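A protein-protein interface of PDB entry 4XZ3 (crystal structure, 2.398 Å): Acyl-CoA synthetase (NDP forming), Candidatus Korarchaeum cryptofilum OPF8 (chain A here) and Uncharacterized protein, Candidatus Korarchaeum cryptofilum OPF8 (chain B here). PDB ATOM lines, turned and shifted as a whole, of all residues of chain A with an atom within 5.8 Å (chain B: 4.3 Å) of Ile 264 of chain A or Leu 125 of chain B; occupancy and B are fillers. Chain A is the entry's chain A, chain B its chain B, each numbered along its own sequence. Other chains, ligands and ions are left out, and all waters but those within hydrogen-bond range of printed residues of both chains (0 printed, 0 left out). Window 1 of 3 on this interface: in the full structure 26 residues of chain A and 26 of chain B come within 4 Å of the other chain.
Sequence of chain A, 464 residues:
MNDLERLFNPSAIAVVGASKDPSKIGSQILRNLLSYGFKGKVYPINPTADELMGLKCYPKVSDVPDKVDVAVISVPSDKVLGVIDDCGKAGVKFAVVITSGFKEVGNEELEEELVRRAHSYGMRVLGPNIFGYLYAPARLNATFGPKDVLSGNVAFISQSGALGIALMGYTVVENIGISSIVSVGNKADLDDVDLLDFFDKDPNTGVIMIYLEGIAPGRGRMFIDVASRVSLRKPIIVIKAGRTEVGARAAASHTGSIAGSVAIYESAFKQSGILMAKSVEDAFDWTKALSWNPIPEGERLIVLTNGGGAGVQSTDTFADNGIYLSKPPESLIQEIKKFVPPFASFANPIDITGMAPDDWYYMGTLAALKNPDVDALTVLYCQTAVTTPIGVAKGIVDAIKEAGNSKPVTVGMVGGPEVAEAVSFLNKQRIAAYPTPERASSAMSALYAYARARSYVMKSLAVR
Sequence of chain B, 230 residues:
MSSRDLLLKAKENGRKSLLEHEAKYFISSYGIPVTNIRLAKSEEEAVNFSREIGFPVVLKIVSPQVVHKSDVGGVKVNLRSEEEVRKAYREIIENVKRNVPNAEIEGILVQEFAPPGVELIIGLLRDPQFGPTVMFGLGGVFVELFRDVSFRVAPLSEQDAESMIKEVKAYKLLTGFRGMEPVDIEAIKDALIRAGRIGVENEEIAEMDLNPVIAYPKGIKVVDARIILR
The backbone carbonyl oxygen (O) of Leu 125 of chain B lies within hydrogen-bond range of the backbone NH (N) of Thr 133 of chain B, at 2.8 Å. The side-chain carboxylate of Asp 127 of chain B is in hydrogen-bond range of the backbone NH of Phe 130 of chain B.
Among the printed residues, pairs that only touch across the chains: Thr 255 of chain A with Leu 124 of chain B, Thr 255 of chain A with Leu 125 of chain B, Gly 256 of chain A with Glu 207 of chain B, Ala 259 of chain A with Leu 125 of chain B, Ile 264 of chain A with Leu 125 of chain B, Ile 264 of chain A with Asp 127 of chain B, Ile 264 of chain A with Phe 130 of chain B, Tyr 265 of chain A with Phe 130 of chain B and Ala 268 of chain A with Phe 130 of chain B.
Printed residues of chain B within 4 Å of Ile 264 of chain A: Leu 125, Asp 127 and Phe 130. Printed residues of chain A within 4 Å of Leu 125 of chain B: Thr 255, Ala 259 and Ile 264. Of the printed residues of chain B, Tyr 265 of chain A touches Phe 130 (3.6 Å). Of the printed residues of chain A, Asp 127 of chain B touches Ile 264 (3.7 Å). Of the printed residues of chain B, Thr 255 of chain A touches Leu 124 and Leu 125. Printed residues of chain A within 4 Å of Glu 207 of chain B: Gly 256. Of the printed residues of chain A, Phe 130 of chain B touches Ile 264 (3.6 Å), Tyr 265 (3.6 Å) and Ala 268 (3.3 Å). The nearest printed residue of chain A that does not touch Leu 125 of chain B is Gly 256 of chain A (4.2 Å). The nearest printed residue of chain B that does not touch Ala 259 of chain A is Thr 133 of chain B (6.9 Å).
Of the 13 printed residues of chain A, 6 touch a printed residue of chain B. Hydrophobic or aromatic side chains of chain A within 4 Å of the printed part of chain B: Ala 259, Ile 264, Tyr 265 and Ala 268. Printed residues of chain B that touch a printed residue of chain A: Leu 124, Leu 125, Asp 127, Phe 130 and Glu 207. Hydrophobic or aromatic side chains of chain B within 4 Å of the printed part of chain A: Leu 125 and Phe 130.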
ATOM      1  N   THR A 255     -22.142   8.631   4.281  1.00  0.00           N
ATOM      2  CA  THR A 255     -21.862   9.843   3.527  1.00  0.00           C
ATOM      3  C   THR A 255     -23.126  10.685   3.441  1.00  0.00           C
ATOM      4  O   THR A 255     -23.104  11.883   3.724  1.00  0.00           O
ATOM      5  CB  THR A 255     -21.342   9.528   2.117  1.00  0.00           C
ATOM      6  OG1 THR A 255     -20.171   8.709   2.219  1.00  0.00           O
ATOM      7  CG2 THR A 255     -20.995  10.812   1.362  1.00  0.00           C
ATOM      8  N   GLY A 256     -24.227  10.044   3.065  1.00  0.00           N
ATOM      9  CA  GLY A 256     -25.507  10.720   2.971  1.00  0.00           C
ATOM     10  C   GLY A 256     -25.927  11.355   4.283  1.00  0.00           C
ATOM     11  O   GLY A 256     -26.544  12.421   4.291  1.00  0.00           O
ATOM     12  N   ALA A 259     -22.924  14.248   5.554  1.00  0.00           N
ATOM     13  CA  ALA A 259     -22.730  15.335   4.599  1.00  0.00           C
ATOM     14  C   ALA A 259     -23.935  16.272   4.600  1.00  0.00           C
ATOM     15  O   ALA A 259     -25.071  15.832   4.417  1.00  0.00           O
ATOM     16  CB  ALA A 259     -22.491  14.788   3.212  1.00  0.00           C
ATOM     17  N   GLY A 260     -23.675  17.558   4.819  1.00  0.00           N
ATOM     18  CA  GLY A 260     -24.713  18.577   4.789  1.00  0.00           C
ATOM     19  C   GLY A 260     -24.424  19.663   3.769  1.00  0.00           C
ATOM     20  O   GLY A 260     -23.260  19.945   3.459  1.00  0.00           O
ATOM     21  N   SER A 261     -25.490  20.274   3.254  1.00  0.00           N
ATOM     22  CA  SER A 261     -25.378  21.303   2.222  1.00  0.00           C
ATOM     23  C   SER A 261     -24.505  22.473   2.675  1.00  0.00           C
ATOM     24  O   SER A 261     -23.797  23.082   1.875  1.00  0.00           O
ATOM     25  CB  SER A 261     -26.763  21.816   1.836  1.00  0.00           C
ATOM     26  OG  SER A 261     -26.679  22.726   0.754  1.00  0.00           O
ATOM     27  N   VAL A 262     -24.563  22.779   3.964  1.00  0.00           N
ATOM     28  CA  VAL A 262     -23.759  23.854   4.530  1.00  0.00           C
ATOM     29  C   VAL A 262     -22.273  23.587   4.328  1.00  0.00           C
ATOM     30  O   VAL A 262     -21.543  24.439   3.817  1.00  0.00           O
ATOM     31  CB  VAL A 262     -24.050  24.026   6.032  1.00  0.00           C
ATOM     32  CG1 VAL A 262     -23.086  25.027   6.670  1.00  0.00           C
ATOM     33  CG2 VAL A 262     -25.494  24.463   6.237  1.00  0.00           C
ATOM     34  N   ALA A 263     -21.833  22.400   4.735  1.00  0.00           N
ATOM     35  CA  ALA A 263     -20.426  22.030   4.642  1.00  0.00           C
ATOM     36  C   ALA A 263     -19.970  21.973   3.188  1.00  0.00           C
ATOM     37  O   ALA A 263     -18.804  22.230   2.882  1.00  0.00           O
ATOM     38  CB  ALA A 263     -20.182  20.694   5.332  1.00  0.00           C
ATOM     39  N   ILE A 264     -20.885  21.632   2.287  1.00  0.00           N
ATOM     40  CA  ILE A 264     -20.534  21.543   0.876  1.00  0.00           C
ATOM     41  C   ILE A 264     -20.372  22.937   0.284  1.00  0.00           C
ATOM     42  O   ILE A 264     -19.483  23.159  -0.538  1.00  0.00           O
ATOM     43  CB  ILE A 264     -21.582  20.743   0.078  1.00  0.00           C
ATOM     44  CG1 ILE A 264     -21.508  19.265   0.484  1.00  0.00           C
ATOM     45  CG2 ILE A 264     -21.342  20.885  -1.428  1.00  0.00           C
ATOM     46  CD1 ILE A 264     -22.529  18.371  -0.189  1.00  0.00           C
ATOM     47  N   TYR A 265     -21.227  23.871   0.693  1.00  0.00           N
ATOM     48  CA  TYR A 265     -21.103  25.252   0.235  1.00  0.00           C
ATOM     49  C   TYR A 265     -19.763  25.827   0.679  1.00  0.00           C
ATOM     50  O   TYR A 265     -19.101  26.526  -0.085  1.00  0.00           O
ATOM     51  CB  TYR A 265     -22.251  26.119   0.762  1.00  0.00           C
ATOM     52  CG  TYR A 265     -23.460  26.181  -0.146  1.00  0.00           C
ATOM     53  CD1 TYR A 265     -23.450  26.944  -1.304  1.00  0.00           C
ATOM     54  CD2 TYR A 265     -24.621  25.493   0.169  1.00  0.00           C
ATOM     55  CE1 TYR A 265     -24.564  27.008  -2.136  1.00  0.00           C
ATOM     56  CE2 TYR A 265     -25.733  25.548  -0.649  1.00  0.00           C
ATOM     57  CZ  TYR A 265     -25.705  26.309  -1.797  1.00  0.00           C
ATOM     58  OH  TYR A 265     -26.834  26.339  -2.589  1.00  0.00           O
ATOM     59  N   GLU A 266     -19.367  25.528   1.914  1.00  0.00           N
ATOM     60  CA  GLU A 266     -18.085  26.003   2.437  1.00  0.00           C
ATOM     61  C   GLU A 266     -16.928  25.500   1.581  1.00  0.00           C
ATOM     62  O   GLU A 266     -16.009  26.252   1.261  1.00  0.00           O
ATOM     63  CB  GLU A 266     -17.894  25.556   3.888  1.00  0.00           C
ATOM     64  CG  GLU A 266     -18.839  26.228   4.872  1.00  0.00           C
ATOM     65  CD  GLU A 266     -18.580  25.821   6.314  1.00  0.00           C
ATOM     66  OE1 GLU A 266     -17.823  24.853   6.538  1.00  0.00           O
ATOM     67  OE2 GLU A 266     -19.132  26.478   7.223  1.00  0.00           O
ATOM     68  N   SER A 267     -16.987  24.231   1.193  1.00  0.00           N
ATOM     69  CA  SER A 267     -15.948  23.633   0.358  1.00  0.00           C
ATOM     70  C   SER A 267     -15.937  24.243  -1.039  1.00  0.00           C
ATOM     71  O   SER A 267     -14.875  24.521  -1.599  1.00  0.00           O
ATOM     72  CB  SER A 267     -16.152  22.124   0.266  1.00  0.00           C
ATOM     73  OG  SER A 267     -16.200  21.554   1.563  1.00  0.00           O
ATOM     74  N   ALA A 268     -17.125  24.444  -1.597  1.00  0.00           N
ATOM     75  CA  ALA A 268     -17.263  25.077  -2.901  1.00  0.00           C
ATOM     76  C   ALA A 268     -16.653  26.479  -2.882  1.00  0.00           C
ATOM     77  O   ALA A 268     -16.003  26.891  -3.843  1.00  0.00           O
ATOM     78  CB  ALA A 268     -18.724  25.136  -3.305  1.00  0.00           C
ATOM     79  N   PHE A 269     -16.865  27.206  -1.787  1.00  0.00           N
ATOM     80  CA  PHE A 269     -16.321  28.554  -1.646  1.00  0.00           C
ATOM     81  C   PHE A 269     -14.802  28.510  -1.527  1.00  0.00           C
ATOM     82  O   PHE A 269     -14.093  29.357  -2.070  1.00  0.00           O
ATOM     83  CB  PHE A 269     -16.931  29.255  -0.425  1.00  0.00           C
ATOM     84  CG  PHE A 269     -18.406  29.540  -0.548  1.00  0.00           C
ATOM     85  CD1 PHE A 269     -18.997  29.750  -1.782  1.00  0.00           C
ATOM     86  CD2 PHE A 269     -19.200  29.612   0.583  1.00  0.00           C
ATOM     87  CE1 PHE A 269     -20.352  30.017  -1.883  1.00  0.00           C
ATOM     88  CE2 PHE A 269     -20.551  29.882   0.486  1.00  0.00           C
ATOM     89  CZ  PHE A 269     -21.127  30.084  -0.749  1.00  0.00           C
ATOM     90  N   LEU B 124     -18.888   9.623  -1.528  1.00  0.00           N
ATOM     91  CA  LEU B 124     -19.267  10.292  -2.759  1.00  0.00           C
ATOM     92  C   LEU B 124     -20.756  10.615  -2.699  1.00  0.00           C
ATOM     93  O   LEU B 124     -21.584   9.719  -2.564  1.00  0.00           O
ATOM     94  CB  LEU B 124     -18.951   9.421  -3.968  1.00  0.00           C
ATOM     95  CG  LEU B 124     -19.250  10.004  -5.343  1.00  0.00           C
ATOM     96  CD1 LEU B 124     -18.247  11.093  -5.711  1.00  0.00           C
ATOM     97  CD2 LEU B 124     -19.250   8.887  -6.364  1.00  0.00           C
ATOM     98  N   LEU B 125     -21.091  11.893  -2.783  1.00  0.00           N
ATOM     99  CA  LEU B 125     -22.477  12.314  -2.670  1.00  0.00           C
ATOM    100  C   LEU B 125     -22.825  13.217  -3.833  1.00  0.00           C
ATOM    101  O   LEU B 125     -22.024  14.053  -4.238  1.00  0.00           O
ATOM    102  CB  LEU B 125     -22.696  13.047  -1.344  1.00  0.00           C
ATOM    103  CG  LEU B 125     -24.074  13.664  -1.098  1.00  0.00           C
ATOM    104  CD1 LEU B 125     -25.100  12.590  -0.791  1.00  0.00           C
ATOM    105  CD2 LEU B 125     -23.999  14.677   0.028  1.00  0.00           C
ATOM    106  N   ARG B 126     -24.045  13.081  -4.338  1.00  0.00           N
ATOM    107  CA  ARG B 126     -24.510  13.940  -5.413  1.00  0.00           C
ATOM    108  C   ARG B 126     -25.321  15.069  -4.806  1.00  0.00           C
ATOM    109  O   ARG B 126     -26.430  14.859  -4.320  1.00  0.00           O
ATOM    110  CB  ARG B 126     -25.337  13.157  -6.430  1.00  0.00           C
ATOM    111  CG  ARG B 126     -25.598  13.942  -7.710  1.00  0.00           C
ATOM    112  CD  ARG B 126     -26.117  13.057  -8.828  1.00  0.00           C
ATOM    113  NE  ARG B 126     -25.185  11.977  -9.136  1.00  0.00           N
ATOM    114  CZ  ARG B 126     -24.131  12.094  -9.939  1.00  0.00           C
ATOM    115  NH1 ARG B 126     -23.858  13.252 -10.530  1.00  0.00           N
ATOM    116  NH2 ARG B 126     -23.344  11.045 -10.152  1.00  0.00           N
ATOM    117  N   ASP B 127     -24.759  16.273  -4.844  1.00  0.00           N
ATOM    118  CA  ASP B 127     -25.451  17.451  -4.345  1.00  0.00           C
ATOM    119  C   ASP B 127     -26.311  18.043  -5.460  1.00  0.00           C
ATOM    120  O   ASP B 127     -25.941  17.968  -6.634  1.00  0.00           O
ATOM    121  CB  ASP B 127     -24.448  18.481  -3.825  1.00  0.00           C
ATOM    122  CG  ASP B 127     -25.116  19.653  -3.136  1.00  0.00           C
ATOM    123  OD1 ASP B 127     -25.597  19.485  -1.992  1.00  0.00           O
ATOM    124  OD2 ASP B 127     -25.151  20.744  -3.736  1.00  0.00           O
ATOM    125  N   PHE B 130     -23.993  21.353  -6.694  1.00  0.00           N
ATOM    126  CA  PHE B 130     -22.637  21.178  -7.211  1.00  0.00           C
ATOM    127  C   PHE B 130     -22.399  19.821  -7.868  1.00  0.00           C
ATOM    128  O   PHE B 130     -21.404  19.633  -8.570  1.00  0.00           O
ATOM    129  CB  PHE B 130     -21.636  21.396  -6.084  1.00  0.00           C
ATOM    130  CG  PHE B 130     -21.812  22.705  -5.385  1.00  0.00           C
ATOM    131  CD1 PHE B 130     -21.238  23.860  -5.892  1.00  0.00           C
ATOM    132  CD2 PHE B 130     -22.567  22.787  -4.232  1.00  0.00           C
ATOM    133  CE1 PHE B 130     -21.408  25.071  -5.254  1.00  0.00           C
ATOM    134  CE2 PHE B 130     -22.738  23.993  -3.588  1.00  0.00           C
ATOM    135  CZ  PHE B 130     -22.158  25.138  -4.099  1.00  0.00           C
ATOM    136  N   GLY B 131     -23.306  18.875  -7.633  1.00  0.00           N
ATOM    137  CA  GLY B 131     -23.196  17.556  -8.225  1.00  0.00           C
ATOM    138  C   GLY B 131     -22.188  16.681  -7.489  1.00  0.00           C
ATOM    139  O   GLY B 131     -22.022  16.826  -6.276  1.00  0.00           O
ATOM    140  N   PRO B 132     -21.504  15.779  -8.216  1.00  0.00           N
ATOM    141  CA  PRO B 132     -20.563  14.830  -7.606  1.00  0.00           C
ATOM    142  C   PRO B 132     -19.588  15.481  -6.630  1.00  0.00           C
ATOM    143  O   PRO B 132     -18.786  16.328  -7.021  1.00  0.00           O
ATOM    144  CB  PRO B 132     -19.821  14.253  -8.813  1.00  0.00           C
ATOM    145  CG  PRO B 132     -20.800  14.342  -9.923  1.00  0.00           C
ATOM    146  CD  PRO B 132     -21.601  15.587  -9.674  1.00  0.00           C
ATOM    147  N   THR B 133     -19.664  15.065  -5.370  1.00  0.00           N
ATOM    148  CA  THR B 133     -18.842  15.617  -4.300  1.00  0.00           C
ATOM    149  C   THR B 133     -18.143  14.484  -3.560  1.00  0.00           C
ATOM    150  O   THR B 133     -18.745  13.448  -3.292  1.00  0.00           O
ATOM    151  CB  THR B 133     -19.692  16.440  -3.305  1.00  0.00           C
ATOM    152  OG1 THR B 133     -20.380  17.486  -4.004  1.00  0.00           O
ATOM    153  CG2 THR B 133     -18.815  17.051  -2.215  1.00  0.00           C
ATOM    154  N   ALA B 206     -26.151   7.932  -6.449  1.00  0.00           N
ATOM    155  CA  ALA B 206     -26.607   8.987  -5.548  1.00  0.00           C
ATOM    156  C   ALA B 206     -25.630   9.166  -4.395  1.00  0.00           C
ATOM    157  O   ALA B 206     -25.168  10.273  -4.120  1.00  0.00           O
ATOM    158  CB  ALA B 206     -27.990   8.666  -5.016  1.00  0.00           C
ATOM    159  N   GLU B 207     -25.332   8.063  -3.719  1.00  0.00           N
ATOM    160  CA  GLU B 207     -24.408   8.066  -2.596  1.00  0.00           C
ATOM    161  C   GLU B 207     -23.466   6.884  -2.738  1.00  0.00           C
ATOM    162  O   GLU B 207     -23.846   5.858  -3.296  1.00  0.00           O
ATOM    163  CB  GLU B 207     -25.161   7.980  -1.266  1.00  0.00           C
ATOM    164  CG  GLU B 207     -26.229   9.041  -1.068  1.00  0.00           C
ATOM    165  CD  GLU B 207     -27.082   8.793   0.168  1.00  0.00           C
ATOM    166  OE1 GLU B 207     -26.665   8.001   1.040  1.00  0.00           O
ATOM    167  OE2 GLU B 207     -28.179   9.382   0.262  1.00  0.00           O
